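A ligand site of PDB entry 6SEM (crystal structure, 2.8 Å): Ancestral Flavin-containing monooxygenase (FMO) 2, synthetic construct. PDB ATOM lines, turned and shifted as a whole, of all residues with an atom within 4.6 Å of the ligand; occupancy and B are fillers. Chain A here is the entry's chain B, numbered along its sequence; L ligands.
An oxygen (O1) of the ligand is in hydrogen-bond range of the backbone NH of Leu 40, at 2.9 Å. N of Arg 33 sits at hydrogen-bond distance from N5 of the ligand, 3.0 Å away. The side-chain amide oxygen (OD1) of Asn 61 lies close to an oxygen (O8) of the ligand (3.1 Å). N7 of the ligand lies within hydrogen-bond range of OG1 of Thr 62 (3.0 Å). The side-chain carboxylate of Glu 32 sits at hydrogen-bond distance from an oxygen (O5) of the ligand. N of Ser 13 lies within hydrogen-bond range of O13 of the ligand, at 3.1 Å. The side-chain hydroxyl of Ser 377 is in hydrogen-bond range of an oxygen (O7) of the ligand (2.7 Å). O of Val 110 sits at hydrogen-bond distance from N3 of the ligand (3.2 Å). A nitrogen (N4) of the ligand sits at hydrogen-bond distance from the backbone NH (N) of Val 110 (3.2 Å). The backbone NH of Val 12 is in hydrogen-bond range of an oxygen (O13) of the ligand. N of Asn 61 lies within hydrogen-bond range of O8 of the ligand (2.6 Å). An oxygen (O10) of the ligand sits at hydrogen-bond distance from a ring nitrogen (ND1) of His 150 (3.3 Å). The backbone NH of Ile 378 sits at hydrogen-bond distance from an oxygen (O7) of the ligand (2.8 Å). The side-chain hydroxyl of Ser 13 is in hydrogen-bond range of an oxygen (O14) of the ligand, at 2.8 Å. NE1 of Trp 41 is in hydrogen-bond range of O9 of the ligand, at 3.1 Å.
The backbone carbonyl oxygen of Phe 31 lies within hydrogen-bond range of the backbone NH of Gly 9 (2.6 Å). N of Ala 10 sits at hydrogen-bond distance from OE1 of Glu 32 (3.1 Å). The backbone carbonyl oxygen of Asp 36 sits at hydrogen-bond distance from the side-chain hydroxyl of Thr 34, at 3.1 Å. The backbone NH of Gly 14 sits close to the side-chain sulfur of Cys 146. The backbone NH (N) of Thr 108 sits at hydrogen-bond distance from the backbone carbonyl oxygen (O) of Glu 32 (3.1 Å). The backbone NH (N) of Phe 379 sits at hydrogen-bond distance from the side-chain hydroxyl (OG) of Ser 377 (3.2 Å). The backbone NH of Cys 146 lies close to the backbone carbonyl oxygen of Ile 8. O of Ile 8 sits at hydrogen-bond distance from N of Ser 147 (3.5 Å).
N5 of the ligand lies close to O of Phe 31, at 3.2 Å. The backbone carbonyl oxygen of Gly 38 sits close to an oxygen (O1) of the ligand (3.5 Å). Ile 8 touches the ligand. Gly 9 touches the ligand (CA to O4, 3.3 Å). Ala 10 touches the ligand. Gly 11 touches the ligand (CA to O13, 3.0 Å). Thr 34 touches the ligand (CG2 to O6, 3.5 Å). Gly 39 touches the ligand (CA to O1, 3.4 Å). Gly 50 touches the ligand. Thr 60 touches the ligand. Thr 108 touches the ligand (O to C9, 3.99 Å). Thr 109 touches the ligand. Cys 146 touches the ligand (O to O4, 3.5 Å). Ser 147 touches the ligand. Gly 148 touches the ligand (CA to O15, 3.5 Å). OG of Ser 195 touches C17 of the ligand (3.96 Å). CD2 of Phe 337 touches N3 of the ligand, at 3.8 Å. CE1 of Phe 379 touches O9 of the ligand, at 3.4 Å. Within 4 Å of the ligand: Ile 8, Gly 9, Ala 10, Gly 11, Val 12, Ser 13, Phe 31, Glu 32, Arg 33, Thr 34, Gly 38, Gly 39, Leu 40, Trp 41, Gly 50, Thr 60, Asn 61, Thr 62, Thr 108, Thr 109, Val 110, Cys 146, Ser 147, Gly 148, His 150, Ser 195, Phe 337, Ser 377, Ile 378 and Phe 379.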
ATOM      1  N   ILE A   8      11.218 -13.182  -0.639  1.00  0.00           N
ATOM      2  CA  ILE A   8      12.423 -12.780   0.074  1.00  0.00           C
ATOM      3  C   ILE A   8      12.024 -12.106   1.390  1.00  0.00           C
ATOM      4  O   ILE A   8      11.553 -10.960   1.395  1.00  0.00           O
ATOM      5  CB  ILE A   8      13.264 -11.789  -0.762  1.00  0.00           C
ATOM      6  CG1 ILE A   8      13.269 -12.100  -2.265  1.00  0.00           C
ATOM      7  CG2 ILE A   8      14.663 -11.699  -0.194  1.00  0.00           C
ATOM      8  CD1 ILE A   8      14.009 -13.356  -2.642  1.00  0.00           C
ATOM      9  N   GLY A   9      12.210 -12.814   2.510  1.00  0.00           N
ATOM     10  CA  GLY A   9      12.004 -12.244   3.843  1.00  0.00           C
ATOM     11  C   GLY A   9      10.645 -12.571   4.431  1.00  0.00           C
ATOM     12  O   GLY A   9       9.630 -12.563   3.732  1.00  0.00           O
ATOM     13  N   ALA A  10      10.628 -12.870   5.741  1.00  0.00           N
ATOM     14  CA  ALA A  10       9.418 -13.174   6.505  1.00  0.00           C
ATOM     15  C   ALA A  10       8.967 -11.924   7.263  1.00  0.00           C
ATOM     16  O   ALA A  10       8.541 -11.998   8.441  1.00  0.00           O
ATOM     17  CB  ALA A  10       9.675 -14.319   7.450  1.00  0.00           C
ATOM     18  N   GLY A  11       9.081 -10.770   6.585  1.00  0.00           N
ATOM     19  CA  GLY A  11       8.556  -9.533   7.083  1.00  0.00           C
ATOM     20  C   GLY A  11       7.053  -9.630   7.228  1.00  0.00           C
ATOM     21  O   GLY A  11       6.489 -10.722   7.258  1.00  0.00           O
ATOM     22  N   VAL A  12       6.405  -8.468   7.329  1.00  0.00           N
ATOM     23  CA  VAL A  12       4.963  -8.410   7.236  1.00  0.00           C
ATOM     24  C   VAL A  12       4.577  -8.703   5.799  1.00  0.00           C
ATOM     25  O   VAL A  12       3.612  -9.415   5.518  1.00  0.00           O
ATOM     26  CB  VAL A  12       4.410  -7.039   7.646  1.00  0.00           C
ATOM     27  CG1 VAL A  12       2.914  -7.149   7.938  1.00  0.00           C
ATOM     28  CG2 VAL A  12       5.183  -6.431   8.803  1.00  0.00           C
ATOM     29  N   SER A  13       5.359  -8.105   4.902  1.00  0.00           N
ATOM     30  CA  SER A  13       5.184  -8.199   3.488  1.00  0.00           C
ATOM     31  C   SER A  13       5.346  -9.666   3.019  1.00  0.00           C
ATOM     32  O   SER A  13       4.484 -10.192   2.326  1.00  0.00           O
ATOM     33  CB  SER A  13       6.125  -7.258   2.803  1.00  0.00           C
ATOM     34  OG  SER A  13       5.959  -5.936   3.297  1.00  0.00           O
ATOM     35  N   GLY A  14       6.419 -10.322   3.453  1.00  0.00           N
ATOM     36  CA  GLY A  14       6.573 -11.758   3.248  1.00  0.00           C
ATOM     37  C   GLY A  14       5.373 -12.553   3.730  1.00  0.00           C
ATOM     38  O   GLY A  14       4.777 -13.334   3.003  1.00  0.00           O
ATOM     39  N   PHE A  31      12.284 -17.202   2.208  1.00  0.00           N
ATOM     40  CA  PHE A  31      13.649 -17.158   2.676  1.00  0.00           C
ATOM     41  C   PHE A  31      13.797 -16.011   3.684  1.00  0.00           C
ATOM     42  O   PHE A  31      13.602 -14.852   3.329  1.00  0.00           O
ATOM     43  CB  PHE A  31      14.610 -16.989   1.506  1.00  0.00           C
ATOM     44  CG  PHE A  31      14.500 -18.077   0.466  1.00  0.00           C
ATOM     45  CD1 PHE A  31      14.654 -19.412   0.821  1.00  0.00           C
ATOM     46  CD2 PHE A  31      14.231 -17.777  -0.860  1.00  0.00           C
ATOM     47  CE1 PHE A  31      14.541 -20.419  -0.132  1.00  0.00           C
ATOM     48  CE2 PHE A  31      14.134 -18.779  -1.820  1.00  0.00           C
ATOM     49  CZ  PHE A  31      14.277 -20.089  -1.452  1.00  0.00           C
ATOM     50  N   GLU A  32      14.221 -16.391   4.897  1.00  0.00           N
ATOM     51  CA  GLU A  32      14.366 -15.483   6.050  1.00  0.00           C
ATOM     52  C   GLU A  32      15.829 -15.412   6.494  1.00  0.00           C
ATOM     53  O   GLU A  32      16.329 -16.420   6.990  1.00  0.00           O
ATOM     54  CB  GLU A  32      13.567 -16.068   7.206  1.00  0.00           C
ATOM     55  CG  GLU A  32      13.807 -15.345   8.506  1.00  0.00           C
ATOM     56  CD  GLU A  32      13.883 -13.859   8.263  1.00  0.00           C
ATOM     57  OE1 GLU A  32      12.910 -13.290   7.755  1.00  0.00           O
ATOM     58  OE2 GLU A  32      14.961 -13.281   8.527  1.00  0.00           O
ATOM     59  N   ARG A  33      16.462 -14.249   6.338  1.00  0.00           N
ATOM     60  CA  ARG A  33      17.878 -14.063   6.750  1.00  0.00           C
ATOM     61  C   ARG A  33      18.042 -14.492   8.226  1.00  0.00           C
ATOM     62  O   ARG A  33      19.011 -15.172   8.567  1.00  0.00           O
ATOM     63  CB  ARG A  33      18.372 -12.614   6.579  1.00  0.00           C
ATOM     64  N   THR A  34      17.064 -14.133   9.056  1.00  0.00           N
ATOM     65  CA  THR A  34      17.136 -14.298  10.505  1.00  0.00           C
ATOM     66  C   THR A  34      16.445 -15.598  10.947  1.00  0.00           C
ATOM     67  O   THR A  34      16.134 -16.451  10.129  1.00  0.00           O
ATOM     68  CB  THR A  34      16.564 -13.053  11.212  1.00  0.00           C
ATOM     69  OG1 THR A  34      15.150 -12.997  10.999  1.00  0.00           O
ATOM     70  CG2 THR A  34      17.214 -11.776  10.725  1.00  0.00           C
ATOM     71  N   ASP A  36      13.574 -15.804  12.760  1.00  0.00           N
ATOM     72  CA  ASP A  36      12.160 -15.631  13.090  1.00  0.00           C
ATOM     73  C   ASP A  36      11.510 -14.557  12.205  1.00  0.00           C
ATOM     74  O   ASP A  36      12.188 -13.764  11.494  1.00  0.00           O
ATOM     75  CB  ASP A  36      11.996 -15.278  14.572  1.00  0.00           C
ATOM     76  CG  ASP A  36      10.612 -15.546  15.165  1.00  0.00           C
ATOM     77  OD1 ASP A  36       9.689 -15.868  14.399  1.00  0.00           O
ATOM     78  OD2 ASP A  36      10.466 -15.393  16.388  1.00  0.00           O
ATOM     79  N   GLY A  38       8.513 -11.382  11.462  1.00  0.00           N
ATOM     80  CA  GLY A  38       8.160 -10.051  11.934  1.00  0.00           C
ATOM     81  C   GLY A  38       8.976  -8.984  11.241  1.00  0.00           C
ATOM     82  O   GLY A  38       8.512  -7.848  10.996  1.00  0.00           O
ATOM     83  N   GLY A  39      10.214  -9.354  10.898  1.00  0.00           N
ATOM     84  CA  GLY A  39      11.188  -8.391  10.475  1.00  0.00           C
ATOM     85  C   GLY A  39      11.257  -7.278  11.500  1.00  0.00           C
ATOM     86  O   GLY A  39      11.456  -7.556  12.677  1.00  0.00           O
ATOM     87  N   LEU A  40      10.997  -6.035  11.050  1.00  0.00           N
ATOM     88  CA  LEU A  40      11.285  -4.820  11.822  1.00  0.00           C
ATOM     89  C   LEU A  40      10.702  -4.907  13.242  1.00  0.00           C
ATOM     90  O   LEU A  40      11.377  -4.527  14.199  1.00  0.00           O
ATOM     91  CB  LEU A  40      10.730  -3.602  11.068  1.00  0.00           C
ATOM     92  CG  LEU A  40      10.545  -2.334  11.893  1.00  0.00           C
ATOM     93  CD1 LEU A  40      10.797  -1.097  11.053  1.00  0.00           C
ATOM     94  CD2 LEU A  40       9.141  -2.276  12.517  1.00  0.00           C
ATOM     95  N   TRP A  41       9.483  -5.439  13.338  1.00  0.00           N
ATOM     96  CA  TRP A  41       8.632  -5.425  14.525  1.00  0.00           C
ATOM     97  C   TRP A  41       9.039  -6.458  15.578  1.00  0.00           C
ATOM     98  O   TRP A  41       8.474  -6.465  16.693  1.00  0.00           O
ATOM     99  CB  TRP A  41       7.180  -5.657  14.096  1.00  0.00           C
ATOM    100  CG  TRP A  41       6.614  -4.498  13.361  1.00  0.00           C
ATOM    101  CD1 TRP A  41       6.442  -4.382  12.016  1.00  0.00           C
ATOM    102  CD2 TRP A  41       6.178  -3.247  13.935  1.00  0.00           C
ATOM    103  NE1 TRP A  41       5.907  -3.158  11.717  1.00  0.00           N
ATOM    104  CE2 TRP A  41       5.738  -2.440  12.876  1.00  0.00           C
ATOM    105  CE3 TRP A  41       6.118  -2.733  15.241  1.00  0.00           C
ATOM    106  CZ2 TRP A  41       5.252  -1.147  13.081  1.00  0.00           C
ATOM    107  CZ3 TRP A  41       5.642  -1.465  15.433  1.00  0.00           C
ATOM    108  CH2 TRP A  41       5.198  -0.688  14.368  1.00  0.00           C
ATOM    109  N   GLY A  50      21.327  -6.395   8.205  1.00  0.00           N
ATOM    110  CA  GLY A  50      20.360  -6.840   7.187  1.00  0.00           C
ATOM    111  C   GLY A  50      18.917  -6.869   7.662  1.00  0.00           C
ATOM    112  O   GLY A  50      18.023  -7.209   6.868  1.00  0.00           O
ATOM    113  N   ARG A  51      18.668  -6.538   8.933  1.00  0.00           N
ATOM    114  CA  ARG A  51      17.296  -6.385   9.456  1.00  0.00           C
ATOM    115  C   ARG A  51      17.155  -5.002  10.092  1.00  0.00           C
ATOM    116  O   ARG A  51      18.108  -4.471  10.652  1.00  0.00           O
ATOM    117  CB  ARG A  51      16.957  -7.433  10.516  1.00  0.00           C
ATOM    118  CG  ARG A  51      15.515  -7.362  10.967  1.00  0.00           C
ATOM    119  CD  ARG A  51      15.047  -8.674  11.575  1.00  0.00           C
ATOM    120  NE  ARG A  51      15.550  -8.879  12.921  1.00  0.00           N
ATOM    121  CZ  ARG A  51      15.033  -8.308  14.003  1.00  0.00           C
ATOM    122  NH1 ARG A  51      14.097  -7.387  13.889  1.00  0.00           N
ATOM    123  NH2 ARG A  51      15.451  -8.682  15.205  1.00  0.00           N
ATOM    124  N   ALA A  52      15.943  -4.453   9.983  1.00  0.00           N
ATOM    125  CA  ALA A  52      15.630  -3.153  10.532  1.00  0.00           C
ATOM    126  C   ALA A  52      15.492  -3.260  12.065  1.00  0.00           C
ATOM    127  O   ALA A  52      14.821  -4.156  12.562  1.00  0.00           O
ATOM    128  CB  ALA A  52      14.374  -2.631   9.886  1.00  0.00           C
ATOM    129  N   TYR A  55      13.802   0.764  18.457  1.00  0.00           N
ATOM    130  CA  TYR A  55      13.878   1.018  19.896  1.00  0.00           C
ATOM    131  C   TYR A  55      12.770   0.238  20.600  1.00  0.00           C
ATOM    132  O   TYR A  55      11.801  -0.150  19.978  1.00  0.00           O
ATOM    133  CB  TYR A  55      13.840   2.531  20.151  1.00  0.00           C
ATOM    134  CG  TYR A  55      12.797   3.303  19.391  1.00  0.00           C
ATOM    135  CD1 TYR A  55      13.122   3.962  18.218  1.00  0.00           C
ATOM    136  CD2 TYR A  55      11.515   3.465  19.886  1.00  0.00           C
ATOM    137  CE1 TYR A  55      12.192   4.726  17.525  1.00  0.00           C
ATOM    138  CE2 TYR A  55      10.565   4.215  19.196  1.00  0.00           C
ATOM    139  CZ  TYR A  55      10.896   4.840  18.008  1.00  0.00           C
ATOM    140  OH  TYR A  55       9.983   5.600  17.339  1.00  0.00           O
ATOM    141  N   VAL A  58       8.456   1.270  20.931  1.00  0.00           N
ATOM    142  CA  VAL A  58       7.685   1.744  19.767  1.00  0.00           C
ATOM    143  C   VAL A  58       6.232   1.287  19.861  1.00  0.00           C
ATOM    144  O   VAL A  58       5.967   0.094  20.069  1.00  0.00           O
ATOM    145  CB  VAL A  58       8.235   1.270  18.417  1.00  0.00           C
ATOM    146  CG1 VAL A  58       7.734   2.177  17.289  1.00  0.00           C
ATOM    147  CG2 VAL A  58       9.756   1.182  18.399  1.00  0.00           C
ATOM    148  N   THR A  60       2.482   1.370  17.606  1.00  0.00           N
ATOM    149  CA  THR A  60       1.947   1.573  16.241  1.00  0.00           C
ATOM    150  C   THR A  60       1.223   2.908  16.167  1.00  0.00           C
ATOM    151  O   THR A  60       0.518   3.208  17.115  1.00  0.00           O
ATOM    152  CB  THR A  60       0.865   0.537  16.000  1.00  0.00           C
ATOM    153  OG1 THR A  60      -0.025   0.766  17.079  1.00  0.00           O
ATOM    154  CG2 THR A  60       1.378  -0.871  16.137  1.00  0.00           C
ATOM    155  N   ASN A  61       1.355   3.655  15.067  1.00  0.00           N
ATOM    156  CA  ASN A  61       0.686   4.903  14.918  1.00  0.00           C
ATOM    157  C   ASN A  61      -0.487   4.745  13.953  1.00  0.00           C
ATOM    158  O   ASN A  61      -0.756   5.666  13.195  1.00  0.00           O
ATOM    159  CB  ASN A  61       1.679   5.978  14.477  1.00  0.00           C
ATOM    160  CG  ASN A  61       2.511   5.578  13.291  1.00  0.00           C
ATOM    161  OD1 ASN A  61       1.986   5.051  12.333  1.00  0.00           O
ATOM    162  ND2 ASN A  61       3.801   5.857  13.335  1.00  0.00           N
ATOM    163  N   THR A  62      -1.145   3.570  13.997  1.00  0.00           N
ATOM    164  CA  THR A  62      -2.400   3.281  13.262  1.00  0.00           C
ATOM    165  C   THR A  62      -3.253   2.270  14.029  1.00  0.00           C
ATOM    166  O   THR A  62      -2.725   1.277  14.544  1.00  0.00           O
ATOM    167  CB  THR A  62      -2.132   2.723  11.862  1.00  0.00           C
ATOM    168  OG1 THR A  62      -1.269   1.595  12.016  1.00  0.00           O
ATOM    169  CG2 THR A  62      -1.541   3.735  10.918  1.00  0.00           C
ATOM    170  N   THR A 108      18.290 -18.736   6.197  1.00  0.00           N
ATOM    171  CA  THR A 108      18.671 -18.864   4.795  1.00  0.00           C
ATOM    172  C   THR A 108      18.521 -17.497   4.133  1.00  0.00           C
ATOM    173  O   THR A 108      17.422 -16.992   3.938  1.00  0.00           O
ATOM    174  CB  THR A 108      17.881 -19.986   4.108  1.00  0.00           C
ATOM    175  OG1 THR A 108      16.494 -19.798   4.384  1.00  0.00           O
ATOM    176  CG2 THR A 108      18.269 -21.370   4.573  1.00  0.00           C
ATOM    177  N   THR A 109      19.659 -16.878   3.803  1.00  0.00           N
ATOM    178  CA  THR A 109      19.711 -15.544   3.215  1.00  0.00           C
ATOM    179  C   THR A 109      19.881 -15.645   1.695  1.00  0.00           C
ATOM    180  O   THR A 109      20.641 -16.479   1.198  1.00  0.00           O
ATOM    181  CB  THR A 109      20.801 -14.681   3.866  1.00  0.00           C
ATOM    182  OG1 THR A 109      21.548 -14.100   2.811  1.00  0.00           O
ATOM    183  CG2 THR A 109      21.731 -15.446   4.798  1.00  0.00           C
ATOM    184  N   VAL A 110      19.166 -14.771   0.968  1.00  0.00           N
ATOM    185  CA  VAL A 110      19.130 -14.773  -0.491  1.00  0.00           C
ATOM    186  C   VAL A 110      20.242 -13.859  -1.025  1.00  0.00           C
ATOM    187  O   VAL A 110      20.205 -12.636  -0.851  1.00  0.00           O
ATOM    188  CB  VAL A 110      17.748 -14.319  -1.001  1.00  0.00           C
ATOM    189  CG1 VAL A 110      17.760 -14.055  -2.496  1.00  0.00           C
ATOM    190  CG2 VAL A 110      16.669 -15.318  -0.630  1.00  0.00           C
ATOM    191  N   CYS A 146      10.444  -8.796  -0.452  1.00  0.00           N
ATOM    192  CA  CYS A 146       9.913  -8.309   0.821  1.00  0.00           C
ATOM    193  C   CYS A 146      11.033  -8.084   1.847  1.00  0.00           C
ATOM    194  O   CYS A 146      10.860  -8.406   3.032  1.00  0.00           O
ATOM    195  CB  CYS A 146       8.911  -9.304   1.399  1.00  0.00           C
ATOM    196  SG  CYS A 146       8.029 -10.241   0.128  1.00  0.00           S
ATOM    197  N   SER A 147      12.151  -7.513   1.400  1.00  0.00           N
ATOM    198  CA  SER A 147      13.349  -7.364   2.233  1.00  0.00           C
ATOM    199  C   SER A 147      13.395  -5.997   2.952  1.00  0.00           C
ATOM    200  O   SER A 147      14.397  -5.706   3.607  1.00  0.00           O
ATOM    201  CB  SER A 147      14.588  -7.582   1.416  1.00  0.00           C
ATOM    202  OG  SER A 147      14.572  -6.758   0.274  1.00  0.00           O
ATOM    203  N   GLY A 148      12.329  -5.190   2.819  1.00  0.00           N
ATOM    204  CA  GLY A 148      12.173  -3.911   3.558  1.00  0.00           C
ATOM    205  C   GLY A 148      13.108  -2.806   3.077  1.00  0.00           C
ATOM    206  O   GLY A 148      13.881  -2.998   2.154  1.00  0.00           O
ATOM    207  N   HIS A 150      13.916   0.139   5.579  1.00  0.00           N
ATOM    208  CA  HIS A 150      14.266   0.891   6.785  1.00  0.00           C
ATOM    209  C   HIS A 150      15.446   0.183   7.484  1.00  0.00           C
ATOM    210  O   HIS A 150      15.480  -0.024   8.708  1.00  0.00           O
ATOM    211  CB  HIS A 150      13.017   0.964   7.678  1.00  0.00           C
ATOM    212  CG  HIS A 150      12.073   2.068   7.354  1.00  0.00           C
ATOM    213  ND1 HIS A 150      10.803   1.811   6.850  1.00  0.00           N
ATOM    214  CD2 HIS A 150      12.174   3.394   7.527  1.00  0.00           C
ATOM    215  CE1 HIS A 150      10.168   2.957   6.712  1.00  0.00           C
ATOM    216  NE2 HIS A 150      10.986   3.952   7.112  1.00  0.00           N
ATOM    217  N   SER A 195      10.301   9.040  14.565  1.00  0.00           N
ATOM    218  CA  SER A 195      11.323   8.411  15.387  1.00  0.00           C
ATOM    219  C   SER A 195      12.066   9.444  16.224  1.00  0.00           C
ATOM    220  O   SER A 195      12.138   9.319  17.419  1.00  0.00           O
ATOM    221  CB  SER A 195      12.248   7.636  14.523  1.00  0.00           C
ATOM    222  OG  SER A 195      11.552   6.536  13.987  1.00  0.00           O
ATOM    223  N   PHE A 337      20.938  -8.110  -3.930  1.00  0.00           N
ATOM    224  CA  PHE A 337      20.809  -9.399  -4.572  1.00  0.00           C
ATOM    225  C   PHE A 337      20.068  -9.248  -5.912  1.00  0.00           C
ATOM    226  O   PHE A 337      19.473 -10.194  -6.396  1.00  0.00           O
ATOM    227  CB  PHE A 337      20.109 -10.378  -3.628  1.00  0.00           C
ATOM    228  CG  PHE A 337      18.792  -9.896  -3.096  1.00  0.00           C
ATOM    229  CD1 PHE A 337      17.640  -9.947  -3.870  1.00  0.00           C
ATOM    230  CD2 PHE A 337      18.699  -9.383  -1.809  1.00  0.00           C
ATOM    231  CE1 PHE A 337      16.422  -9.505  -3.374  1.00  0.00           C
ATOM    232  CE2 PHE A 337      17.485  -8.915  -1.328  1.00  0.00           C
ATOM    233  CZ  PHE A 337      16.357  -8.965  -2.106  1.00  0.00           C
ATOM    234  N   GLY A 376      -1.566   5.871   5.300  1.00  0.00           N
ATOM    235  CA  GLY A 376      -2.257   5.008   6.226  1.00  0.00           C
ATOM    236  C   GLY A 376      -1.420   3.785   6.513  1.00  0.00           C
ATOM    237  O   GLY A 376      -0.240   3.769   6.250  1.00  0.00           O
ATOM    238  N   SER A 377      -2.041   2.743   7.059  1.00  0.00           N
ATOM    239  CA  SER A 377      -1.301   1.588   7.482  1.00  0.00           C
ATOM    240  C   SER A 377      -0.744   0.850   6.265  1.00  0.00           C
ATOM    241  O   SER A 377      -1.399   0.714   5.230  1.00  0.00           O
ATOM    242  CB  SER A 377      -2.141   0.706   8.337  1.00  0.00           C
ATOM    243  OG  SER A 377      -1.453  -0.496   8.614  1.00  0.00           O
ATOM    244  N   ILE A 378       0.473   0.341   6.425  1.00  0.00           N
ATOM    245  CA  ILE A 378       1.112  -0.417   5.370  1.00  0.00           C
ATOM    246  C   ILE A 378       0.481  -1.807   5.269  1.00  0.00           C
ATOM    247  O   ILE A 378       0.523  -2.413   4.224  1.00  0.00           O
ATOM    248  CB  ILE A 378       2.632  -0.507   5.592  1.00  0.00           C
ATOM    249  CG1 ILE A 378       3.396  -0.357   4.278  1.00  0.00           C
ATOM    250  CG2 ILE A 378       3.003  -1.799   6.288  1.00  0.00           C
ATOM    251  CD1 ILE A 378       4.881  -0.324   4.502  1.00  0.00           C
ATOM    252  N   PHE A 379      -0.074  -2.323   6.360  1.00  0.00           N
ATOM    253  CA  PHE A 379      -0.440  -3.740   6.400  1.00  0.00           C
ATOM    254  C   PHE A 379      -1.541  -4.034   5.377  1.00  0.00           C
ATOM    255  O   PHE A 379      -1.413  -4.992   4.625  1.00  0.00           O
ATOM    256  CB  PHE A 379      -0.771  -4.181   7.829  1.00  0.00           C
ATOM    257  CG  PHE A 379       0.261  -3.783   8.854  1.00  0.00           C
ATOM    258  CD1 PHE A 379       1.611  -3.799   8.537  1.00  0.00           C
ATOM    259  CD2 PHE A 379      -0.109  -3.362  10.111  1.00  0.00           C
ATOM    260  CE1 PHE A 379       2.570  -3.392   9.462  1.00  0.00           C
ATOM    261  CE2 PHE A 379       0.841  -2.950  11.036  1.00  0.00           C
ATOM    262  CZ  PHE A 379       2.180  -2.969  10.705  1.00  0.00           C
HETATM  263  P1  LIG L   1      10.826  -5.733   7.162  1.00  0.00           P
HETATM  264  O1  LIG L   1       9.930  -6.135   8.338  1.00  0.00           O
HETATM  265  O2  LIG L   1      12.100  -4.895   7.227  1.00  0.00           O
HETATM  266  O3  LIG L   1      11.269  -7.104   6.475  1.00  0.00           O
HETATM  267  C1  LIG L   1      12.611  -7.561   6.517  1.00  0.00           C
HETATM  268  C2  LIG L   1      12.567  -9.090   6.614  1.00  0.00           C
HETATM  269  O4  LIG L   1      13.141  -9.625   5.427  1.00  0.00           O
HETATM  270  C3  LIG L   1      13.386  -9.580   7.788  1.00  0.00           C
HETATM  271  O5  LIG L   1      12.847 -10.821   8.276  1.00  0.00           O
HETATM  272  C4  LIG L   1      14.750  -9.671   7.148  1.00  0.00           C
HETATM  273  O6  LIG L   1      15.691 -10.532   7.795  1.00  0.00           O
HETATM  274  C5  LIG L   1      14.368 -10.248   5.798  1.00  0.00           C
HETATM  275  N1  LIG L   1      15.454 -10.079   4.804  1.00  0.00           N
HETATM  276  C6  LIG L   1      16.147  -8.971   4.496  1.00  0.00           C
HETATM  277  N2  LIG L   1      17.077  -9.260   3.551  1.00  0.00           N
HETATM  278  C7  LIG L   1      16.972 -10.572   3.297  1.00  0.00           C
HETATM  279  C8  LIG L   1      17.634 -11.535   2.420  1.00  0.00           C
HETATM  280  N3  LIG L   1      18.633 -11.171   1.585  1.00  0.00           N
HETATM  281  N4  LIG L   1      17.206 -12.810   2.481  1.00  0.00           N
HETATM  282  C9  LIG L   1      16.228 -13.245   3.287  1.00  0.00           C
HETATM  283  N5  LIG L   1      15.579 -12.422   4.101  1.00  0.00           N
HETATM  284  C10 LIG L   1      15.913 -11.110   4.118  1.00  0.00           C
HETATM  285  N6  LIG L   1       3.201   0.857   9.449  1.00  0.00           N
HETATM  286  C11 LIG L   1       1.931   0.868   9.920  1.00  0.00           C
HETATM  287  O7  LIG L   1       1.007   0.491   9.185  1.00  0.00           O
HETATM  288  N7  LIG L   1       1.584   1.262  11.147  1.00  0.00           N
HETATM  289  C12 LIG L   1       2.507   1.693  12.016  1.00  0.00           C
HETATM  290  O8  LIG L   1       2.161   2.066  13.156  1.00  0.00           O
HETATM  291  C13 LIG L   1       3.936   1.729  11.581  1.00  0.00           C
HETATM  292  N8  LIG L   1       4.920   2.138  12.419  1.00  0.00           N
HETATM  293  C14 LIG L   1       6.212   2.163  12.022  1.00  0.00           C
HETATM  294  C15 LIG L   1       7.150   2.615  12.950  1.00  0.00           C
HETATM  295  C16 LIG L   1       8.489   2.679  12.614  1.00  0.00           C
HETATM  296  C17 LIG L   1       9.490   3.181  13.618  1.00  0.00           C
HETATM  297  C18 LIG L   1       8.930   2.260  11.269  1.00  0.00           C
HETATM  298  C19 LIG L   1      10.396   2.348  10.945  1.00  0.00           C
HETATM  299  C20 LIG L   1       8.003   1.805  10.332  1.00  0.00           C
HETATM  300  C21 LIG L   1       6.632   1.739  10.651  1.00  0.00           C
HETATM  301  N9  LIG L   1       5.615   1.275   9.743  1.00  0.00           N
HETATM  302  C22 LIG L   1       4.260   1.275  10.202  1.00  0.00           C
HETATM  303  C23 LIG L   1       5.925   0.818   8.360  1.00  0.00           C
HETATM  304  C24 LIG L   1       6.093  -0.709   8.279  1.00  0.00           C
HETATM  305  O9  LIG L   1       5.277  -1.343   9.277  1.00  0.00           O
HETATM  306  C25 LIG L   1       7.523  -1.170   8.498  1.00  0.00           C
HETATM  307  O10 LIG L   1       8.423  -0.373   7.705  1.00  0.00           O
HETATM  308  C26 LIG L   1       7.652  -2.712   8.300  1.00  0.00           C
HETATM  309  O11 LIG L   1       9.024  -3.043   8.455  1.00  0.00           O
HETATM  310  C27 LIG L   1       7.252  -3.388   7.002  1.00  0.00           C
HETATM  311  O12 LIG L   1       7.682  -4.778   6.987  1.00  0.00           O
HETATM  312  P2  LIG L   1       8.450  -5.482   5.722  1.00  0.00           P
HETATM  313  O13 LIG L   1       8.115  -6.964   5.696  1.00  0.00           O
HETATM  314  O14 LIG L   1       8.232  -4.724   4.447  1.00  0.00           O
HETATM  315  O15 LIG L   1       9.989  -5.119   5.954  1.00  0.00           O
